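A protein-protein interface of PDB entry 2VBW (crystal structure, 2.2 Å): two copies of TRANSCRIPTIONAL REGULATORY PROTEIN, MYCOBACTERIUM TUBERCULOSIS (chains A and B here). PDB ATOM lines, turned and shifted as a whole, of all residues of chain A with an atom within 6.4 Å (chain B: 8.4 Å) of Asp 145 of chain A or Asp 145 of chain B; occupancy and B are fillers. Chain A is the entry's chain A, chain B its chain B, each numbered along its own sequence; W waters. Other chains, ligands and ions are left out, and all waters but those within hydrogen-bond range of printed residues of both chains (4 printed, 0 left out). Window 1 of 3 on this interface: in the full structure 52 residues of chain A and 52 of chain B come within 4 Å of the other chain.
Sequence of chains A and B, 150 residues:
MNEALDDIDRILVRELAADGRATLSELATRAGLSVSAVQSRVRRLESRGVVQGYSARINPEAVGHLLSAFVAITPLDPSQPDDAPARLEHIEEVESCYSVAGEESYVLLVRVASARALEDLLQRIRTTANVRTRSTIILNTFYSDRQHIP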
ATOM      1  N   ALA A  17     -27.124 -17.554 -32.860  1.00  0.00           N
ATOM      2  CA  ALA A  17     -26.167 -17.647 -31.720  1.00  0.00           C
ATOM      3  C   ALA A  17     -26.831 -18.047 -30.390  1.00  0.00           C
ATOM      4  O   ALA A  17     -26.264 -18.839 -29.621  1.00  0.00           O
ATOM      5  CB  ALA A  17     -25.368 -16.327 -31.536  1.00  0.00           C
ATOM      6  N   SER A  55     -23.224 -26.157 -32.813  1.00  0.00           N
ATOM      7  CA  SER A  55     -22.856 -27.200 -31.838  1.00  0.00           C
ATOM      8  C   SER A  55     -23.791 -27.173 -30.691  1.00  0.00           C
ATOM      9  O   SER A  55     -24.218 -26.098 -30.314  1.00  0.00           O
ATOM     10  CB  SER A  55     -21.464 -26.928 -31.219  1.00  0.00           C
ATOM     11  OG  SER A  55     -20.532 -26.654 -32.220  1.00  0.00           O
ATOM     12  N   ARG A  57     -23.766 -27.175 -26.794  1.00  0.00           N
ATOM     13  CA  ARG A  57     -22.847 -26.821 -25.705  1.00  0.00           C
ATOM     14  C   ARG A  57     -22.862 -27.922 -24.638  1.00  0.00           C
ATOM     15  O   ARG A  57     -23.835 -28.037 -23.882  1.00  0.00           O
ATOM     16  CB  ARG A  57     -23.258 -25.525 -25.080  1.00  0.00           C
ATOM     17  N   GLU A  95      -8.633 -28.085 -26.857  1.00  0.00           N
ATOM     18  CA  GLU A  95      -9.880 -27.588 -27.394  1.00  0.00           C
ATOM     19  C   GLU A  95      -9.713 -26.309 -28.242  1.00  0.00           C
ATOM     20  O   GLU A  95     -10.508 -26.076 -29.162  1.00  0.00           O
ATOM     21  CB  GLU A  95     -10.808 -27.362 -26.223  1.00  0.00           C
ATOM     22  CG  GLU A  95     -12.115 -26.644 -26.558  1.00  0.00           C
ATOM     23  CD  GLU A  95     -13.137 -26.706 -25.410  1.00  0.00           C
ATOM     24  OE1 GLU A  95     -13.687 -25.606 -25.077  1.00  0.00           O
ATOM     25  OE2 GLU A  95     -13.367 -27.836 -24.832  1.00  0.00           O
ATOM     26  N   SER A  96      -8.705 -25.466 -27.931  1.00  0.00           N
ATOM     27  CA  SER A  96      -8.421 -24.253 -28.709  1.00  0.00           C
ATOM     28  C   SER A  96      -6.969 -23.873 -28.686  1.00  0.00           C
ATOM     29  O   SER A  96      -6.213 -24.200 -27.748  1.00  0.00           O
ATOM     30  CB  SER A  96      -9.098 -23.047 -28.117  1.00  0.00           C
ATOM     31  OG  SER A  96     -10.337 -23.372 -27.610  1.00  0.00           O
ATOM     32  N   TYR A  98      -4.621 -20.380 -29.824  1.00  0.00           N
ATOM     33  CA  TYR A  98      -4.509 -19.008 -30.303  1.00  0.00           C
ATOM     34  C   TYR A  98      -3.040 -18.610 -30.341  1.00  0.00           C
ATOM     35  O   TYR A  98      -2.287 -19.034 -29.477  1.00  0.00           O
ATOM     36  CB  TYR A  98      -5.173 -18.046 -29.293  1.00  0.00           C
ATOM     37  CG  TYR A  98      -6.571 -18.408 -28.915  1.00  0.00           C
ATOM     38  CD1 TYR A  98      -6.836 -19.205 -27.810  1.00  0.00           C
ATOM     39  CD2 TYR A  98      -7.662 -17.902 -29.658  1.00  0.00           C
ATOM     40  CE1 TYR A  98      -8.140 -19.562 -27.457  1.00  0.00           C
ATOM     41  CE2 TYR A  98      -8.965 -18.244 -29.331  1.00  0.00           C
ATOM     42  CZ  TYR A  98      -9.208 -19.061 -28.227  1.00  0.00           C
ATOM     43  OH  TYR A  98     -10.538 -19.367 -27.917  1.00  0.00           O
ATOM     44  N   ARG A 111      -8.562 -29.743 -21.694  1.00  0.00           N
ATOM     45  CA  ARG A 111      -9.460 -30.399 -20.728  1.00  0.00           C
ATOM     46  C   ARG A 111      -9.101 -31.828 -20.534  1.00  0.00           C
ATOM     47  O   ARG A 111      -8.888 -32.549 -21.493  1.00  0.00           O
ATOM     48  CB  ARG A 111     -10.928 -30.308 -21.137  1.00  0.00           C
ATOM     49  CG  ARG A 111     -11.370 -28.864 -21.325  1.00  0.00           C
ATOM     50  CD  ARG A 111     -12.830 -28.714 -21.263  1.00  0.00           C
ATOM     51  NE  ARG A 111     -13.283 -27.501 -21.950  1.00  0.00           N
ATOM     52  CZ  ARG A 111     -13.637 -26.365 -21.347  1.00  0.00           C
ATOM     53  NH1 ARG A 111     -13.517 -26.245 -20.027  1.00  0.00           N
ATOM     54  NH2 ARG A 111     -14.126 -25.368 -22.082  1.00  0.00           N
ATOM     55  N   TYR A 143     -19.237 -18.163 -16.805  1.00  0.00           N
ATOM     56  CA  TYR A 143     -20.047 -18.174 -18.018  1.00  0.00           C
ATOM     57  C   TYR A 143     -19.052 -18.192 -19.155  1.00  0.00           C
ATOM     58  O   TYR A 143     -17.864 -17.823 -18.999  1.00  0.00           O
ATOM     59  CB  TYR A 143     -21.023 -16.959 -18.088  1.00  0.00           C
ATOM     60  CG  TYR A 143     -20.485 -15.621 -17.584  1.00  0.00           C
ATOM     61  CD1 TYR A 143     -20.673 -15.220 -16.260  1.00  0.00           C
ATOM     62  CD2 TYR A 143     -19.816 -14.739 -18.442  1.00  0.00           C
ATOM     63  CE1 TYR A 143     -20.149 -13.967 -15.782  1.00  0.00           C
ATOM     64  CE2 TYR A 143     -19.314 -13.465 -17.970  1.00  0.00           C
ATOM     65  CZ  TYR A 143     -19.471 -13.124 -16.640  1.00  0.00           C
ATOM     66  OH  TYR A 143     -18.948 -11.915 -16.147  1.00  0.00           O
ATOM     67  N   SER A 144     -19.498 -18.650 -20.307  1.00  0.00           N
ATOM     68  CA  SER A 144     -18.612 -18.811 -21.441  1.00  0.00           C
ATOM     69  C   SER A 144     -19.402 -18.745 -22.715  1.00  0.00           C
ATOM     70  O   SER A 144     -20.631 -18.869 -22.698  1.00  0.00           O
ATOM     71  CB  SER A 144     -17.816 -20.123 -21.358  1.00  0.00           C
ATOM     72  OG  SER A 144     -18.648 -21.201 -21.007  1.00  0.00           O
ATOM     73  N   ASP A 145     -18.682 -18.495 -23.797  1.00  0.00           N
ATOM     74  CA  ASP A 145     -19.185 -18.558 -25.142  1.00  0.00           C
ATOM     75  C   ASP A 145     -20.413 -17.685 -25.317  1.00  0.00           C
ATOM     76  O   ASP A 145     -21.280 -17.983 -26.127  1.00  0.00           O
ATOM     77  CB  ASP A 145     -19.472 -20.021 -25.587  1.00  0.00           C
ATOM     78  CG  ASP A 145     -18.223 -20.942 -25.489  1.00  0.00           C
ATOM     79  OD1 ASP A 145     -17.124 -20.575 -25.981  1.00  0.00           O
ATOM     80  OD2 ASP A 145     -18.337 -22.040 -24.883  1.00  0.00           O
ATOM     81  N   ARG A 146     -20.489 -16.587 -24.594  1.00  0.00           N
ATOM     82  CA  ARG A 146     -21.584 -15.709 -24.842  1.00  0.00           C
ATOM     83  C   ARG A 146     -21.328 -14.713 -25.971  1.00  0.00           C
ATOM     84  O   ARG A 146     -20.794 -13.666 -25.758  1.00  0.00           O
ATOM     85  CB  ARG A 146     -22.141 -15.145 -23.559  1.00  0.00           C
ATOM     86  CG  ARG A 146     -21.627 -13.922 -23.138  1.00  0.00           C
ATOM     87  CD  ARG A 146     -21.259 -14.110 -21.701  1.00  0.00           C
ATOM     88  NE  ARG A 146     -22.188 -13.512 -20.782  1.00  0.00           N
ATOM     89  CZ  ARG A 146     -22.122 -12.281 -20.263  1.00  0.00           C
ATOM     90  NH1 ARG A 146     -21.179 -11.388 -20.581  1.00  0.00           N
ATOM     91  NH2 ARG A 146     -23.036 -11.948 -19.373  1.00  0.00           N
ATOM     92  N   GLN A 147     -21.714 -15.123 -27.188  1.00  0.00           N
ATOM     93  CA  GLN A 147     -21.391 -14.437 -28.450  1.00  0.00           C
ATOM     94  C   GLN A 147     -22.172 -13.155 -28.581  1.00  0.00           C
ATOM     95  O   GLN A 147     -23.352 -13.138 -28.338  1.00  0.00           O
ATOM     96  CB  GLN A 147     -21.648 -15.334 -29.654  1.00  0.00           C
ATOM     97  CG  GLN A 147     -20.746 -16.525 -29.746  1.00  0.00           C
ATOM     98  CD  GLN A 147     -21.129 -17.451 -30.898  1.00  0.00           C
ATOM     99  OE1 GLN A 147     -20.479 -17.428 -31.937  1.00  0.00           O
ATOM    100  NE2 GLN A 147     -22.162 -18.300 -30.700  1.00  0.00           N
ATOM    101  N   ALA B  17     -22.495 -32.292 -30.640  1.00  0.00           N
ATOM    102  CA  ALA B  17     -21.318 -31.428 -30.520  1.00  0.00           C
ATOM    103  C   ALA B  17     -20.743 -31.142 -31.891  1.00  0.00           C
ATOM    104  O   ALA B  17     -20.381 -30.022 -32.175  1.00  0.00           O
ATOM    105  CB  ALA B  17     -20.249 -32.065 -29.620  1.00  0.00           C
ATOM    106  N   ALA B  18     -20.657 -32.153 -32.741  1.00  0.00           N
ATOM    107  CA  ALA B  18     -20.133 -31.932 -34.089  1.00  0.00           C
ATOM    108  C   ALA B  18     -21.122 -31.195 -34.990  1.00  0.00           C
ATOM    109  O   ALA B  18     -20.694 -30.399 -35.805  1.00  0.00           O
ATOM    110  CB  ALA B  18     -19.698 -33.235 -34.737  1.00  0.00           C
ATOM    111  N   GLN B  52     -26.305 -28.011 -22.638  1.00  0.00           N
ATOM    112  CA  GLN B  52     -26.614 -26.744 -22.015  1.00  0.00           C
ATOM    113  C   GLN B  52     -27.243 -25.731 -22.949  1.00  0.00           C
ATOM    114  O   GLN B  52     -27.658 -24.677 -22.496  1.00  0.00           O
ATOM    115  CB  GLN B  52     -25.330 -26.108 -21.487  1.00  0.00           C
ATOM    116  CG  GLN B  52     -24.489 -26.999 -20.575  1.00  0.00           C
ATOM    117  CD  GLN B  52     -23.394 -26.202 -19.906  1.00  0.00           C
ATOM    118  OE1 GLN B  52     -23.477 -25.922 -18.711  1.00  0.00           O
ATOM    119  NE2 GLN B  52     -22.372 -25.804 -20.678  1.00  0.00           N
ATOM    120  N   SER B  55     -25.744 -23.627 -30.282  1.00  0.00           N
ATOM    121  CA  SER B  55     -25.444 -22.307 -30.798  1.00  0.00           C
ATOM    122  C   SER B  55     -24.866 -22.387 -32.204  1.00  0.00           C
ATOM    123  O   SER B  55     -24.245 -23.382 -32.585  1.00  0.00           O
ATOM    124  CB  SER B  55     -24.491 -21.444 -29.762  1.00  0.00           C
ATOM    125  N   ALA B  56     -25.139 -21.380 -33.004  1.00  0.00           N
ATOM    126  CA  ALA B  56     -24.396 -21.217 -34.232  1.00  0.00           C
ATOM    127  C   ALA B  56     -23.036 -20.633 -33.798  1.00  0.00           C
ATOM    128  O   ALA B  56     -22.990 -19.790 -32.909  1.00  0.00           O
ATOM    129  CB  ALA B  56     -25.099 -20.247 -35.155  1.00  0.00           C
ATOM    130  N   ARG B  57     -21.959 -21.080 -34.433  1.00  0.00           N
ATOM    131  CA  ARG B  57     -20.619 -20.498 -34.194  1.00  0.00           C
ATOM    132  C   ARG B  57     -20.377 -19.339 -35.147  1.00  0.00           C
ATOM    133  O   ARG B  57     -20.209 -19.531 -36.336  1.00  0.00           O
ATOM    134  CB  ARG B  57     -19.537 -21.583 -34.292  1.00  0.00           C
ATOM    135  CG  ARG B  57     -19.649 -22.614 -33.125  1.00  0.00           C
ATOM    136  CD  ARG B  57     -18.901 -23.944 -33.403  1.00  0.00           C
ATOM    137  NE  ARG B  57     -17.450 -23.693 -33.583  1.00  0.00           N
ATOM    138  CZ  ARG B  57     -16.778 -23.875 -34.727  1.00  0.00           C
ATOM    139  NH1 ARG B  57     -17.411 -24.356 -35.812  1.00  0.00           N
ATOM    140  NH2 ARG B  57     -15.468 -23.586 -34.787  1.00  0.00           N
ATOM    141  N   ILE B  58     -20.445 -18.124 -34.631  1.00  0.00           N
ATOM    142  CA  ILE B  58     -20.319 -16.948 -35.470  1.00  0.00           C
ATOM    143  C   ILE B  58     -18.841 -16.497 -35.593  1.00  0.00           C
ATOM    144  O   ILE B  58     -18.116 -16.439 -34.614  1.00  0.00           O
ATOM    145  CB  ILE B  58     -21.162 -15.775 -34.892  1.00  0.00           C
ATOM    146  CG1 ILE B  58     -22.592 -16.227 -34.536  1.00  0.00           C
ATOM    147  CG2 ILE B  58     -21.146 -14.566 -35.838  1.00  0.00           C
ATOM    148  CD1 ILE B  58     -23.382 -16.959 -35.672  1.00  0.00           C
ATOM    149  N   VAL B  94     -17.682  -9.077 -22.871  1.00  0.00           N
ATOM    150  CA  VAL B  94     -17.103 -10.217 -22.193  1.00  0.00           C
ATOM    151  C   VAL B  94     -17.775 -11.532 -22.563  1.00  0.00           C
ATOM    152  O   VAL B  94     -18.901 -11.805 -22.217  1.00  0.00           O
ATOM    153  CB  VAL B  94     -16.685 -10.003 -20.654  1.00  0.00           C
ATOM    154  CG1 VAL B  94     -17.227  -8.775 -20.046  1.00  0.00           C
ATOM    155  CG2 VAL B  94     -16.822 -11.277 -19.798  1.00  0.00           C
ATOM    156  N   GLU B  95     -17.059 -12.316 -23.340  1.00  0.00           N
ATOM    157  CA  GLU B  95     -17.567 -13.556 -23.822  1.00  0.00           C
ATOM    158  C   GLU B  95     -17.493 -14.683 -22.780  1.00  0.00           C
ATOM    159  O   GLU B  95     -18.380 -15.548 -22.726  1.00  0.00           O
ATOM    160  CB  GLU B  95     -16.824 -13.926 -25.093  1.00  0.00           C
ATOM    161  CG  GLU B  95     -17.288 -15.230 -25.722  1.00  0.00           C
ATOM    162  CD  GLU B  95     -16.831 -15.344 -27.159  1.00  0.00           C
ATOM    163  OE1 GLU B  95     -16.384 -16.431 -27.490  1.00  0.00           O
ATOM    164  OE2 GLU B  95     -16.936 -14.354 -27.950  1.00  0.00           O
ATOM    165  N   SER B  96     -16.458 -14.655 -21.947  1.00  0.00           N
ATOM    166  CA  SER B  96     -16.198 -15.708 -20.959  1.00  0.00           C
ATOM    167  C   SER B  96     -15.537 -15.121 -19.723  1.00  0.00           C
ATOM    168  O   SER B  96     -14.777 -14.166 -19.851  1.00  0.00           O
ATOM    169  CB  SER B  96     -15.247 -16.742 -21.522  1.00  0.00           C
ATOM    170  OG  SER B  96     -15.747 -17.239 -22.730  1.00  0.00           O
ATOM    171  N   CYS B  97     -15.763 -15.749 -18.560  1.00  0.00           N
ATOM    172  CA  CYS B  97     -15.103 -15.370 -17.320  1.00  0.00           C
ATOM    173  C   CYS B  97     -14.761 -16.618 -16.508  1.00  0.00           C
ATOM    174  O   CYS B  97     -15.606 -17.455 -16.263  1.00  0.00           O
ATOM    175  CB  CYS B  97     -16.036 -14.450 -16.531  1.00  0.00           C
ATOM    176  SG  CYS B  97     -15.444 -13.940 -14.994  1.00  0.00           S
ATOM    177  N   TYR B  98     -13.512 -16.740 -16.083  1.00  0.00           N
ATOM    178  CA  TYR B  98     -13.019 -17.923 -15.346  1.00  0.00           C
ATOM    179  C   TYR B  98     -12.269 -17.438 -14.135  1.00  0.00           C
ATOM    180  O   TYR B  98     -11.532 -16.468 -14.259  1.00  0.00           O
ATOM    181  CB  TYR B  98     -11.983 -18.682 -16.205  1.00  0.00           C
ATOM    182  CG  TYR B  98     -12.435 -19.093 -17.589  1.00  0.00           C
ATOM    183  CD1 TYR B  98     -12.206 -18.258 -18.712  1.00  0.00           C
ATOM    184  CD2 TYR B  98     -13.008 -20.362 -17.811  1.00  0.00           C
ATOM    185  CE1 TYR B  98     -12.577 -18.650 -19.997  1.00  0.00           C
ATOM    186  CE2 TYR B  98     -13.434 -20.766 -19.125  1.00  0.00           C
ATOM    187  CZ  TYR B  98     -13.221 -19.885 -20.193  1.00  0.00           C
ATOM    188  OH  TYR B  98     -13.555 -20.251 -21.466  1.00  0.00           O
ATOM    189  N   LEU B 109     -12.354 -13.484 -21.701  1.00  0.00           N
ATOM    190  CA  LEU B 109     -12.138 -13.410 -23.117  1.00  0.00           C
ATOM    191  C   LEU B 109     -13.080 -12.315 -23.571  1.00  0.00           C
ATOM    192  O   LEU B 109     -14.253 -12.328 -23.278  1.00  0.00           O
ATOM    193  CB  LEU B 109     -12.393 -14.717 -23.832  1.00  0.00           C
ATOM    194  CG  LEU B 109     -12.334 -14.694 -25.373  1.00  0.00           C
ATOM    195  CD1 LEU B 109     -11.019 -14.257 -25.815  1.00  0.00           C
ATOM    196  CD2 LEU B 109     -12.534 -16.101 -25.908  1.00  0.00           C
ATOM    197  N   ARG B 111     -13.972  -9.311 -26.789  1.00  0.00           N
ATOM    198  CA  ARG B 111     -13.954  -9.029 -28.235  1.00  0.00           C
ATOM    199  C   ARG B 111     -14.469  -7.628 -28.537  1.00  0.00           C
ATOM    200  O   ARG B 111     -15.437  -7.172 -27.943  1.00  0.00           O
ATOM    201  CB  ARG B 111     -14.772 -10.055 -29.032  1.00  0.00           C
ATOM    202  CG  ARG B 111     -14.521 -11.473 -28.620  1.00  0.00           C
ATOM    203  CD  ARG B 111     -14.412 -12.291 -29.818  1.00  0.00           C
ATOM    204  NE  ARG B 111     -14.533 -13.692 -29.467  1.00  0.00           N
ATOM    205  CZ  ARG B 111     -13.638 -14.613 -29.785  1.00  0.00           C
ATOM    206  NH1 ARG B 111     -12.540 -14.286 -30.497  1.00  0.00           N
ATOM    207  NH2 ARG B 111     -13.861 -15.878 -29.413  1.00  0.00           N
ATOM    208  N   THR B 141      -6.786 -17.016 -34.355  1.00  0.00           N
ATOM    209  CA  THR B 141      -7.380 -18.219 -33.754  1.00  0.00           C
ATOM    210  C   THR B 141      -7.217 -19.395 -34.688  1.00  0.00           C
ATOM    211  O   THR B 141      -7.787 -19.370 -35.737  1.00  0.00           O
ATOM    212  CB  THR B 141      -8.847 -17.992 -33.467  1.00  0.00           C
ATOM    213  OG1 THR B 141      -8.931 -16.946 -32.518  1.00  0.00           O
ATOM    214  CG2 THR B 141      -9.527 -19.226 -32.866  1.00  0.00           C
ATOM    215  N   PHE B 142      -6.459 -20.423 -34.318  1.00  0.00           N
ATOM    216  CA  PHE B 142      -6.227 -21.544 -35.228  1.00  0.00           C
ATOM    217  C   PHE B 142      -7.351 -22.543 -35.220  1.00  0.00           C
ATOM    218  O   PHE B 142      -7.706 -23.041 -36.275  1.00  0.00           O
ATOM    219  CB  PHE B 142      -4.884 -22.255 -34.988  1.00  0.00           C
ATOM    220  CG  PHE B 142      -3.731 -21.399 -35.318  1.00  0.00           C
ATOM    221  CD1 PHE B 142      -3.264 -20.458 -34.377  1.00  0.00           C
ATOM    222  CD2 PHE B 142      -3.150 -21.453 -36.594  1.00  0.00           C
ATOM    223  CE1 PHE B 142      -2.175 -19.589 -34.684  1.00  0.00           C
ATOM    224  CE2 PHE B 142      -2.074 -20.575 -36.930  1.00  0.00           C
ATOM    225  CZ  PHE B 142      -1.588 -19.638 -35.960  1.00  0.00           C
ATOM    226  N   TYR B 143      -7.891 -22.851 -34.042  1.00  0.00           N
ATOM    227  CA  TYR B 143      -9.135 -23.594 -33.938  1.00  0.00           C
ATOM    228  C   TYR B 143      -9.572 -23.337 -32.551  1.00  0.00           C
ATOM    229  O   TYR B 143      -8.721 -23.047 -31.720  1.00  0.00           O
ATOM    230  CB  TYR B 143      -8.924 -25.103 -34.173  1.00  0.00           C
ATOM    231  CG  TYR B 143      -7.604 -25.684 -33.669  1.00  0.00           C
ATOM    232  CD1 TYR B 143      -6.485 -25.695 -34.483  1.00  0.00           C
ATOM    233  CD2 TYR B 143      -7.489 -26.231 -32.385  1.00  0.00           C
ATOM    234  CE1 TYR B 143      -5.290 -26.222 -34.047  1.00  0.00           C
ATOM    235  CE2 TYR B 143      -6.308 -26.803 -31.951  1.00  0.00           C
ATOM    236  CZ  TYR B 143      -5.221 -26.781 -32.804  1.00  0.00           C
ATOM    237  OH  TYR B 143      -3.998 -27.299 -32.432  1.00  0.00           O
ATOM    238  N   SER B 144     -10.882 -23.358 -32.320  1.00  0.00           N
ATOM    239  CA  SER B 144     -11.470 -23.179 -31.019  1.00  0.00           C
ATOM    240  C   SER B 144     -12.700 -24.101 -30.854  1.00  0.00           C
ATOM    241  O   SER B 144     -13.254 -24.600 -31.833  1.00  0.00           O
ATOM    242  CB  SER B 144     -11.843 -21.707 -30.779  1.00  0.00           C
ATOM    243  OG  SER B 144     -12.762 -21.240 -31.755  1.00  0.00           O
ATOM    244  N   ASP B 145     -13.104 -24.347 -29.617  1.00  0.00           N
ATOM    245  CA  ASP B 145     -14.299 -25.127 -29.362  1.00  0.00           C
ATOM    246  C   ASP B 145     -14.330 -26.539 -29.945  1.00  0.00           C
ATOM    247  O   ASP B 145     -15.410 -27.006 -30.290  1.00  0.00           O
ATOM    248  CB  ASP B 145     -15.494 -24.377 -29.947  1.00  0.00           C
ATOM    249  CG  ASP B 145     -16.129 -23.484 -28.952  1.00  0.00           C
ATOM    250  OD1 ASP B 145     -16.903 -24.024 -28.085  1.00  0.00           O
ATOM    251  OD2 ASP B 145     -15.831 -22.262 -29.027  1.00  0.00           O
ATOM    252  N   ARG B 146     -13.184 -27.210 -30.088  1.00  0.00           N
ATOM    253  CA  ARG B 146     -13.206 -28.593 -30.484  1.00  0.00           C
ATOM    254  C   ARG B 146     -13.545 -29.395 -29.224  1.00  0.00           C
ATOM    255  O   ARG B 146     -12.656 -29.867 -28.513  1.00  0.00           O
ATOM    256  CB  ARG B 146     -11.891 -29.080 -31.111  1.00  0.00           C
ATOM    257  CG  ARG B 146     -11.068 -28.088 -31.936  1.00  0.00           C
ATOM    258  CD  ARG B 146     -10.171 -28.806 -32.968  1.00  0.00           C
ATOM    259  NE  ARG B 146      -8.872 -29.456 -32.621  1.00  0.00           N
ATOM    260  CZ  ARG B 146      -8.537 -29.995 -31.461  1.00  0.00           C
ATOM    261  NH1 ARG B 146      -9.412 -29.981 -30.474  1.00  0.00           N
ATOM    262  NH2 ARG B 146      -7.352 -30.583 -31.273  1.00  0.00           N
ATOM    263  N   GLN B 147     -14.832 -29.536 -28.947  1.00  0.00           N
ATOM    264  CA  GLN B 147     -15.323 -30.319 -27.801  1.00  0.00           C
ATOM    265  C   GLN B 147     -14.998 -31.783 -27.976  1.00  0.00           C
ATOM    266  O   GLN B 147     -15.311 -32.377 -29.009  1.00  0.00           O
ATOM    267  CB  GLN B 147     -16.822 -30.106 -27.576  1.00  0.00           C
ATOM    268  CG  GLN B 147     -17.154 -28.690 -27.159  1.00  0.00           C
ATOM    269  CD  GLN B 147     -18.630 -28.431 -27.053  1.00  0.00           C
ATOM    270  OE1 GLN B 147     -19.141 -28.170 -25.960  1.00  0.00           O
ATOM    271  NE2 GLN B 147     -19.329 -28.445 -28.194  1.00  0.00           N
ATOM    272  N   HIS B 148     -14.308 -32.337 -26.974  1.00  0.00           N
ATOM    273  CA  HIS B 148     -13.827 -33.710 -27.014  1.00  0.00           C
ATOM    274  C   HIS B 148     -14.677 -34.554 -26.064  1.00  0.00           C
ATOM    275  O   HIS B 148     -14.918 -34.160 -24.906  1.00  0.00           O
ATOM    276  CB  HIS B 148     -12.335 -33.784 -26.664  1.00  0.00           C
ATOM    277  CG  HIS B 148     -11.835 -35.178 -26.448  1.00  0.00           C
ATOM    278  ND1 HIS B 148     -12.006 -36.186 -27.384  1.00  0.00           N
ATOM    279  CD2 HIS B 148     -11.187 -35.739 -25.396  1.00  0.00           C
ATOM    280  CE1 HIS B 148     -11.483 -37.308 -26.912  1.00  0.00           C
ATOM    281  NE2 HIS B 148     -10.967 -37.061 -25.716  1.00  0.00           N
HETATM  282  O   HOH W   1     -12.600 -18.375 -29.370  1.00  0.00           O
HETATM  283  O   HOH W   2     -14.759 -22.590 -21.899  1.00  0.00           O
HETATM  284  O   HOH W   3     -18.201 -15.176 -31.617  1.00  0.00           O
HETATM  285  O   HOH W   4     -13.344 -30.417 -24.684  1.00  0.00           O
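The side-chain hydroxyl (OG) of Ser 55 of chain A is in hydrogen-bond range of the backbone carbonyl oxygen (O) of Ala 17 of chain B, at 3.4 Å. N of Ser 55 of chain B lies within hydrogen-bond range of O of Ser 55 of chain A (2.9 Å). N of Gln 52 of chain B sits at hydrogen-bond distance from O of Arg 57 of chain A (2.8 Å). O of Glu 95 of chain A sits at hydrogen-bond distance from N of Asp 145 of chain B (3.2 Å). N of Arg 146 of chain B sits at hydrogen-bond distance from O of Glu 95 of chain A. The backbone carbonyl oxygen (O) of Tyr 143 of chain A is in hydrogen-bond range of the backbone NH (N) of Cys 97 of chain B (3.0 Å). The backbone NH (N) of Asp 145 of chain A is in hydrogen-bond range of the backbone carbonyl oxygen (O) of Glu 95 of chain B (3.2 Å). OG of Ser 96 of chain B sits at hydrogen-bond distance from N of Asp 145 of chain A, 3.4 Å away. The backbone carbonyl oxygen (O) of Val 94 of chain B lies within hydrogen-bond range of the guanidinium group (NH1) of Arg 146 of chain A (2.8 Å). The backbone NH (N) of Arg 146 of chain A sits at hydrogen-bond distance from the backbone carbonyl oxygen (O) of Glu 95 of chain B. The side-chain amide nitrogen (NE2) of Gln 147 of chain A lies within hydrogen-bond range of the backbone carbonyl oxygen (O) of Ala 56 of chain B (2.8 Å). The side-chain amide oxygen of Gln 147 of chain A is in hydrogen-bond range of the backbone NH of Ile 58 of chain B (2.8 Å).
Asp 145 of chain A touches three residues of chain B. Of chain A, only Glu 95, Ser 96 and Asp 145 come within 4 Å of Asp 145 of chain B. Ser 144 of chain A touches just these residues of chain B: Glu 95 and Ser 96. Of the printed residues of chain A, Arg 146 of chain B touches Glu 95. Printed residues of chain A within 4 Å of Thr 141 of chain B: Tyr 98 (3.3 Å). Printed residues of chain A within 4 Å of Ser 96 of chain B: Tyr 143 (3.3 Å), Ser 144 (3.5 Å) and Asp 145 (3.4 Å). Of the printed residues of chain B, Gln 147 of chain A touches Ala 56 (2.8 Å), Arg 57 (3.7 Å) and Ile 58 (2.8 Å). The nearest printed residue of chain A that does not touch Arg 146 of chain B is Ser 96 of chain A (5.2 Å).
Water W4 bridges the side-chain carboxylate of Glu 95 of chain A and the backbone NH of His 148 of chain B. Water W2 lies within hydrogen-bond range of OH of Tyr 98 of chain B (2.7 Å) and NH2 of Arg 111 of chain A (2.9 Å). Water W1 bridges the side-chain hydroxyl (OH) of Tyr 98 of chain A (2.7 Å) and the guanidinium group (NH2) of Arg 111 of chain B (2.8 Å). Water W3 bridges OE1 of Gln 147 of chain A (3.2 Å) and O of Ile 58 of chain B (3.3 Å).
Glu 95 of chain A touches Ser 144 of chain B, and with the chains exchanged Ser 144 of chain A touches Glu 95 of chain B. Ser 96 of chain A touches Tyr 143 of chain B, and with the chains exchanged Tyr 143 of chain A touches Ser 96 of chain B. Ser 96 of chain A touches Ser 144 of chain B, and with the chains exchanged Ser 144 of chain A touches Ser 96 of chain B. 12 positions are printed for both chains.
Arg 57 of chain B touches Ser 55 of chain A (CD to OG, 3.4 Å). Ser 144 of chain B touches Ser 96 of chain A. Tyr 98 of chain A touches Ser 144 of chain B (OH to CB, 3.9 Å). Tyr 143 of chain A touches Val 94 of chain B (CE2 to CG2, 3.8 Å). Tyr 143 of chain A touches Ser 96 of chain B (O to CA, 3.3 Å). C of Ser 144 of chain A touches O of Glu 95 of chain B, 3.4 Å away. Asp 145 of chain B touches Asp 145 of chain A (OD2 to OD1, 3.7 Å).
Of the 12 printed residues of chain A, 11 touch a printed residue of chain B. Printed residues of chain A that touch a printed residue of chain B: Ala 17, Ser 55, Arg 57, Glu 95, Ser 96, Tyr 98, Tyr 143, Ser 144, Asp 145, Arg 146 and Gln 147. Of the 22 printed residues of chain B, 16 touch a printed residue of chain A. Hydrophobic or aromatic side chains of chain B that line the printed part of chain A: Ile 58 and Val 94. Among the printed residues, no Asp or Glu carboxylate lies within 4 Å of a Lys or Arg side-chain nitrogen of the other chain.
The side-chain carboxylate (OE2) of Glu 95 of chain A lies within salt-bridge range of the guanidinium group (NE) of Arg 111 of chain A (2.9 Å). The backbone NH (N) of Glu 95 of chain B is in hydrogen-bond range of the backbone carbonyl oxygen (O) of Leu 109 of chain B. NE of Arg 111 of chain B is in salt-bridge range of OE2 of Glu 95 of chain B (2.9 Å). O of Ser 96 of chain B sits at hydrogen-bond distance from N of Leu 109 of chain B, 3.1 Å away.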
